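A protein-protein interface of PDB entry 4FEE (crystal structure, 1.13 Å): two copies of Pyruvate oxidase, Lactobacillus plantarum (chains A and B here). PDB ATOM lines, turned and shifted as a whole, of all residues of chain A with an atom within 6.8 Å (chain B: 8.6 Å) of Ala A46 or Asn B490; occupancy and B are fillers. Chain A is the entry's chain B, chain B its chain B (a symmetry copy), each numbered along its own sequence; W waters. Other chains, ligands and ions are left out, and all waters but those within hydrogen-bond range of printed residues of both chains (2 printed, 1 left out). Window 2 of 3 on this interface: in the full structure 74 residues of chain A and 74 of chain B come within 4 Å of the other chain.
OD2 of Asp A42 is in hydrogen-bond range of N of Gln B489, at 2.9 Å. The side-chain carboxylate (OD1) of Asp A42 sits at hydrogen-bond distance from the backbone NH (N) of Asn B490 (2.8 Å). The side-chain hydroxyl (OG) of Ser A45 is in hydrogen-bond range of the backbone carbonyl oxygen (O) of Asp B491. O of Phe B492 is in hydrogen-bond range of NH2 of Arg A48 (2.7 Å).
O of Ser A45 is in hydrogen-bond range of NE of Arg A48. N of Ile B493 sits at hydrogen-bond distance from OE1 of Gln B484, at 3.0 Å. The side-chain amide oxygen (OD1) of Asn B488 lies within hydrogen-bond range of the side-chain hydroxyl (OG1) of Thr B487 (2.8 Å).
Met A41 touches Ile B493. CB of Asn B488 touches OD1 of Asp A42, at 3.5 Å. Leu A44 touches Ile B493 (CB to CD1, 3.98 Å). Ser A45 touches Asn B490. Ser A45 touches Ile B493 (CA to CD1, 3.8 Å). Ala A46 touches Asn B490. Arg A48 touches Ile B493.
Ala A46 touches just one residue of chain B: Asn B490 (3.6 Å). Glu A47 touches none of the printed residues of chain B. Printed residues of chain B within 4 Å of Arg A48: Phe B492 (2.7 Å) and Ile B493 (3.6 Å). Glu B485 touches none of the printed residues of chain A. Printed residues of chain A within 4 Å of Asn B488: Asp A42. Asn B490 touches three residues of chain A. The nearest printed residue of chain B that does not touch Ala A46 is Ile B493 (6.1 Å).
Printed residues of chain A that touch a printed residue of chain B: Met A41, Asp A42, Leu A44, Ser A45, Ala A46 and Arg A48. Of the 10 printed residues of chain B, 6 touch a printed residue of chain A.
No position is printed for both chains.
Water W1 lies within hydrogen-bond range of OD2 of Asp A42 and OE1 of Gln B489. Water W2 bridges OG of Ser A45 (2.9 Å) and N of Asp B491 (3.0 Å).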
ATOM      1  N   LEU A  12      -1.405   4.255 -15.755  1.00  0.00           N
ATOM      2  CA  LEU A  12      -0.664   4.580 -16.983  1.00  0.00           C
ATOM      3  C   LEU A  12       0.819   4.537 -16.725  1.00  0.00           C
ATOM      4  O   LEU A  12       1.306   5.049 -15.686  1.00  0.00           O
ATOM      5  CB  LEU A  12      -1.052   5.965 -17.500  1.00  0.00           C
ATOM      6  CG  LEU A  12      -2.460   6.087 -18.043  1.00  0.00           C
ATOM      7  CD1 LEU A  12      -2.746   7.536 -18.400  1.00  0.00           C
ATOM      8  CD2 LEU A  12      -2.687   5.271 -19.285  1.00  0.00           C
ATOM      9  N   MET A  41       4.284  14.567 -21.171  1.00  0.00           N
ATOM     10  CA  MET A  41       3.672  15.833 -20.827  1.00  0.00           C
ATOM     11  C   MET A  41       2.317  15.615 -20.152  1.00  0.00           C
ATOM     12  O   MET A  41       1.967  16.284 -19.190  1.00  0.00           O
ATOM     13  CB  MET A  41       3.469  16.740 -22.066  1.00  0.00           C
ATOM     14  CG  MET A  41       4.716  17.191 -22.815  1.00  0.00           C
ATOM     15  SD  MET A  41       5.996  17.838 -21.800  1.00  0.00           S
ATOM     16  CE  MET A  41       5.176  19.198 -21.037  1.00  0.00           C
ATOM     17  N   ASP A  42       1.516  14.682 -20.694  1.00  0.00           N
ATOM     18  CA  ASP A  42       0.189  14.403 -20.170  1.00  0.00           C
ATOM     19  C   ASP A  42       0.280  13.980 -18.713  1.00  0.00           C
ATOM     20  O   ASP A  42      -0.549  14.381 -17.896  1.00  0.00           O
ATOM     21  CB  ASP A  42      -0.511  13.386 -21.037  1.00  0.00           C
ATOM     22  CG  ASP A  42      -1.996  13.477 -21.099  1.00  0.00           C
ATOM     23  OD1 ASP A  42      -2.561  14.521 -20.687  1.00  0.00           O
ATOM     24  OD2 ASP A  42      -2.618  12.505 -21.618  1.00  0.00           O
ATOM     25  N   ALA A  43       1.273  13.145 -18.383  1.00  0.00           N
ATOM     26  CA  ALA A  43       1.449  12.681 -17.001  1.00  0.00           C
ATOM     27  C   ALA A  43       1.895  13.809 -16.090  1.00  0.00           C
ATOM     28  O   ALA A  43       1.408  13.926 -14.953  1.00  0.00           O
ATOM     29  CB  ALA A  43       2.408  11.526 -16.971  1.00  0.00           C
ATOM     30  N   LEU A  44       2.774  14.670 -16.576  1.00  0.00           N
ATOM     31  CA  LEU A  44       3.183  15.863 -15.814  1.00  0.00           C
ATOM     32  C   LEU A  44       1.993  16.762 -15.505  1.00  0.00           C
ATOM     33  O   LEU A  44       1.880  17.355 -14.464  1.00  0.00           O
ATOM     34  CB  LEU A  44       4.259  16.639 -16.545  1.00  0.00           C
ATOM     35  CG  LEU A  44       5.639  16.011 -16.597  1.00  0.00           C
ATOM     36  CD1 LEU A  44       6.524  16.776 -17.570  1.00  0.00           C
ATOM     37  CD2 LEU A  44       6.263  16.009 -15.215  1.00  0.00           C
ATOM     38  N   SER A  45       1.090  16.885 -16.482  1.00  0.00           N
ATOM     39  CA  SER A  45      -0.014  17.804 -16.364  1.00  0.00           C
ATOM     40  C   SER A  45      -0.927  17.451 -15.218  1.00  0.00           C
ATOM     41  O   SER A  45      -1.522  18.344 -14.603  1.00  0.00           O
ATOM     42  CB  SER A  45      -0.787  17.835 -17.694  1.00  0.00           C
ATOM     43  OG  SER A  45      -1.853  18.701 -17.615  1.00  0.00           O
ATOM     44  N   ALA A  46      -1.046  16.167 -14.924  1.00  0.00           N
ATOM     45  CA  ALA A  46      -1.871  15.700 -13.817  1.00  0.00           C
ATOM     46  C   ALA A  46      -1.212  15.814 -12.442  1.00  0.00           C
ATOM     47  O   ALA A  46      -1.866  15.648 -11.448  1.00  0.00           O
ATOM     48  CB  ALA A  46      -2.254  14.245 -14.067  1.00  0.00           C
ATOM     49  N   GLU A  47       0.082  16.109 -12.431  1.00  0.00           N
ATOM     50  CA  GLU A  47       0.902  16.164 -11.216  1.00  0.00           C
ATOM     51  C   GLU A  47       1.544  17.494 -10.896  1.00  0.00           C
ATOM     52  O   GLU A  47       2.563  17.599 -10.247  1.00  0.00           O
ATOM     53  CB  GLU A  47       1.984  15.082 -11.328  1.00  0.00           C
ATOM     54  CG  GLU A  47       1.465  13.674 -11.253  1.00  0.00           C
ATOM     55  CD  GLU A  47       1.033  13.340  -9.843  1.00  0.00           C
ATOM     56  OE1 GLU A  47       1.704  13.572  -8.823  1.00  0.00           O
ATOM     57  OE2 GLU A  47      -0.096  12.821  -9.726  1.00  0.00           O
ATOM     58  N   ARG A  48       0.883  18.588 -11.281  1.00  0.00           N
ATOM     59  CA  ARG A  48       1.397  19.907 -10.989  1.00  0.00           C
ATOM     60  C   ARG A  48       1.542  20.255  -9.521  1.00  0.00           C
ATOM     61  O   ARG A  48       2.399  21.117  -9.254  1.00  0.00           O
ATOM     62  CB  ARG A  48       0.461  20.943 -11.627  1.00  0.00           C
ATOM     63  CG  ARG A  48       0.454  20.729 -13.140  1.00  0.00           C
ATOM     64  CD  ARG A  48      -0.529  21.731 -13.713  1.00  0.00           C
ATOM     65  NE  ARG A  48      -0.662  21.465 -15.146  1.00  0.00           N
ATOM     66  CZ  ARG A  48      -0.567  22.390 -16.106  1.00  0.00           C
ATOM     67  NH1 ARG A  48       0.035  23.562 -15.968  1.00  0.00           N
ATOM     68  NH2 ARG A  48      -0.962  22.152 -17.304  1.00  0.00           N
ATOM     69  N   ASP A  49       0.786  19.657  -8.626  1.00  0.00           N
ATOM     70  CA  ASP A  49       1.020  20.067  -7.220  1.00  0.00           C
ATOM     71  C   ASP A  49       2.322  19.504  -6.710  1.00  0.00           C
ATOM     72  O   ASP A  49       2.942  20.062  -5.831  1.00  0.00           O
ATOM     73  CB  ASP A  49      -0.188  19.612  -6.403  1.00  0.00           C
ATOM     74  CG  ASP A  49      -0.086  20.148  -4.984  1.00  0.00           C
ATOM     75  OD1 ASP A  49      -0.245  19.273  -4.118  1.00  0.00           O
ATOM     76  OD2 ASP A  49       0.177  21.354  -4.777  1.00  0.00           O
ATOM     77  N   GLN B 484      -1.777  18.335 -28.560  1.00  0.00           N
ATOM     78  CA  GLN B 484      -2.279  18.037 -27.221  1.00  0.00           C
ATOM     79  C   GLN B 484      -3.793  18.023 -27.155  1.00  0.00           C
ATOM     80  O   GLN B 484      -4.408  17.182 -26.495  1.00  0.00           O
ATOM     81  CB  GLN B 484      -1.747  18.999 -26.143  1.00  0.00           C
ATOM     82  CG  GLN B 484      -0.272  18.906 -25.914  1.00  0.00           C
ATOM     83  CD  GLN B 484       0.263  19.684 -24.775  1.00  0.00           C
ATOM     84  OE1 GLN B 484      -0.458  20.491 -24.156  1.00  0.00           O
ATOM     85  NE2 GLN B 484       1.542  19.489 -24.460  1.00  0.00           N
ATOM     86  N   GLU B 485      -4.445  18.948 -27.898  1.00  0.00           N
ATOM     87  CA  GLU B 485      -5.897  18.939 -27.949  1.00  0.00           C
ATOM     88  C   GLU B 485      -6.393  17.585 -28.462  1.00  0.00           C
ATOM     89  O   GLU B 485      -7.390  17.032 -28.014  1.00  0.00           O
ATOM     90  CB  GLU B 485      -6.387  20.078 -28.833  1.00  0.00           C
ATOM     91  CG  GLU B 485      -7.934  20.171 -28.892  1.00  0.00           C
ATOM     92  CD  GLU B 485      -8.299  21.286 -29.817  1.00  0.00           C
ATOM     93  OE1 GLU B 485      -8.180  22.492 -29.455  1.00  0.00           O
ATOM     94  OE2 GLU B 485      -8.775  20.948 -30.968  1.00  0.00           O
ATOM     95  N   ASP B 486      -5.699  17.067 -29.451  1.00  0.00           N
ATOM     96  CA  ASP B 486      -6.110  15.833 -30.122  1.00  0.00           C
ATOM     97  C   ASP B 486      -5.832  14.580 -29.308  1.00  0.00           C
ATOM     98  O   ASP B 486      -6.605  13.622 -29.351  1.00  0.00           O
ATOM     99  CB  ASP B 486      -5.443  15.739 -31.495  1.00  0.00           C
ATOM    100  CG  ASP B 486      -5.908  16.744 -32.520  1.00  0.00           C
ATOM    101  OD1 ASP B 486      -6.978  17.393 -32.312  1.00  0.00           O
ATOM    102  OD2 ASP B 486      -5.234  16.947 -33.558  1.00  0.00           O
ATOM    103  N   THR B 487      -4.711  14.526 -28.569  1.00  0.00           N
ATOM    104  CA  THR B 487      -4.288  13.302 -27.913  1.00  0.00           C
ATOM    105  C   THR B 487      -4.317  13.291 -26.405  1.00  0.00           C
ATOM    106  O   THR B 487      -4.392  12.215 -25.827  1.00  0.00           O
ATOM    107  CB  THR B 487      -2.834  12.947 -28.287  1.00  0.00           C
ATOM    108  OG1 THR B 487      -1.929  14.016 -27.922  1.00  0.00           O
ATOM    109  CG2 THR B 487      -2.658  12.727 -29.776  1.00  0.00           C
ATOM    110  N   ASN B 488      -4.169  14.414 -25.761  1.00  0.00           N
ATOM    111  CA  ASN B 488      -3.866  14.416 -24.317  1.00  0.00           C
ATOM    112  C   ASN B 488      -5.110  14.408 -23.516  1.00  0.00           C
ATOM    113  O   ASN B 488      -6.117  15.075 -23.846  1.00  0.00           O
ATOM    114  CB  ASN B 488      -2.995  15.620 -23.964  1.00  0.00           C
ATOM    115  CG  ASN B 488      -1.549  15.424 -24.356  1.00  0.00           C
ATOM    116  OD1 ASN B 488      -1.218  14.756 -25.330  1.00  0.00           O
ATOM    117  ND2 ASN B 488      -0.622  15.998 -23.577  1.00  0.00           N
ATOM    118  N   GLN B 489      -5.128  13.637 -22.444  1.00  0.00           N
ATOM    119  CA  GLN B 489      -6.203  13.516 -21.483  1.00  0.00           C
ATOM    120  C   GLN B 489      -6.332  14.766 -20.622  1.00  0.00           C
ATOM    121  O   GLN B 489      -7.439  15.245 -20.352  1.00  0.00           O
ATOM    122  CB  GLN B 489      -5.987  12.305 -20.559  1.00  0.00           C
ATOM    123  CG  GLN B 489      -7.052  12.183 -19.483  1.00  0.00           C
ATOM    124  CD  GLN B 489      -6.847  10.976 -18.588  1.00  0.00           C
ATOM    125  OE1 GLN B 489      -5.694  10.503 -18.376  1.00  0.00           O
ATOM    126  NE2 GLN B 489      -8.006  10.538 -18.137  1.00  0.00           N
ATOM    127  N   ASN B 490      -5.205  15.223 -20.128  1.00  0.00           N
ATOM    128  CA  ASN B 490      -5.097  16.268 -19.104  1.00  0.00           C
ATOM    129  C   ASN B 490      -4.922  17.614 -19.782  1.00  0.00           C
ATOM    130  O   ASN B 490      -4.871  17.776 -20.988  1.00  0.00           O
ATOM    131  CB  ASN B 490      -3.998  15.908 -18.112  1.00  0.00           C
ATOM    132  CG  ASN B 490      -4.259  14.541 -17.500  1.00  0.00           C
ATOM    133  OD1 ASN B 490      -5.385  14.303 -17.023  1.00  0.00           O
ATOM    134  ND2 ASN B 490      -3.312  13.641 -17.492  1.00  0.00           N
ATOM    135  N   ASP B 491      -4.847  18.653 -18.987  1.00  0.00           N
ATOM    136  CA  ASP B 491      -4.816  20.027 -19.438  1.00  0.00           C
ATOM    137  C   ASP B 491      -3.565  20.311 -20.282  1.00  0.00           C
ATOM    138  O   ASP B 491      -2.520  19.689 -20.115  1.00  0.00           O
ATOM    139  CB  ASP B 491      -4.845  20.999 -18.268  1.00  0.00           C
ATOM    140  CG  ASP B 491      -6.047  21.047 -17.371  1.00  0.00           C
ATOM    141  OD1 ASP B 491      -6.962  20.246 -17.656  1.00  0.00           O
ATOM    142  OD2 ASP B 491      -6.128  21.805 -16.370  1.00  0.00           O
ATOM    143  N   PHE B 492      -3.667  21.307 -21.183  1.00  0.00           N
ATOM    144  CA  PHE B 492      -2.544  21.809 -21.948  1.00  0.00           C
ATOM    145  C   PHE B 492      -1.364  22.073 -21.010  1.00  0.00           C
ATOM    146  O   PHE B 492      -1.560  22.603 -19.909  1.00  0.00           O
ATOM    147  CB  PHE B 492      -2.905  23.114 -22.657  1.00  0.00           C
ATOM    148  CG  PHE B 492      -3.897  22.973 -23.777  1.00  0.00           C
ATOM    149  CD1 PHE B 492      -3.674  22.101 -24.817  1.00  0.00           C
ATOM    150  CD2 PHE B 492      -5.066  23.750 -23.795  1.00  0.00           C
ATOM    151  CE1 PHE B 492      -4.570  22.045 -25.860  1.00  0.00           C
ATOM    152  CE2 PHE B 492      -5.979  23.660 -24.837  1.00  0.00           C
ATOM    153  CZ  PHE B 492      -5.726  22.799 -25.876  1.00  0.00           C
ATOM    154  N   ILE B 493      -0.184  21.761 -21.485  1.00  0.00           N
ATOM    155  CA  ILE B 493       1.012  21.998 -20.657  1.00  0.00           C
ATOM    156  C   ILE B 493       2.187  22.312 -21.599  1.00  0.00           C
ATOM    157  O   ILE B 493       2.477  21.634 -22.567  1.00  0.00           O
ATOM    158  CB  ILE B 493       1.309  20.803 -19.757  1.00  0.00           C
ATOM    159  CG1 ILE B 493       2.506  21.078 -18.858  1.00  0.00           C
ATOM    160  CG2 ILE B 493       1.419  19.476 -20.513  1.00  0.00           C
ATOM    161  CD1 ILE B 493       2.647  20.086 -17.715  1.00  0.00           C
HETATM  162  O   HOH W   1      -3.309  10.362 -20.001  1.00  0.00           O
HETATM  163  O   HOH W   2      -4.261  18.489 -16.048  1.00  0.00           O
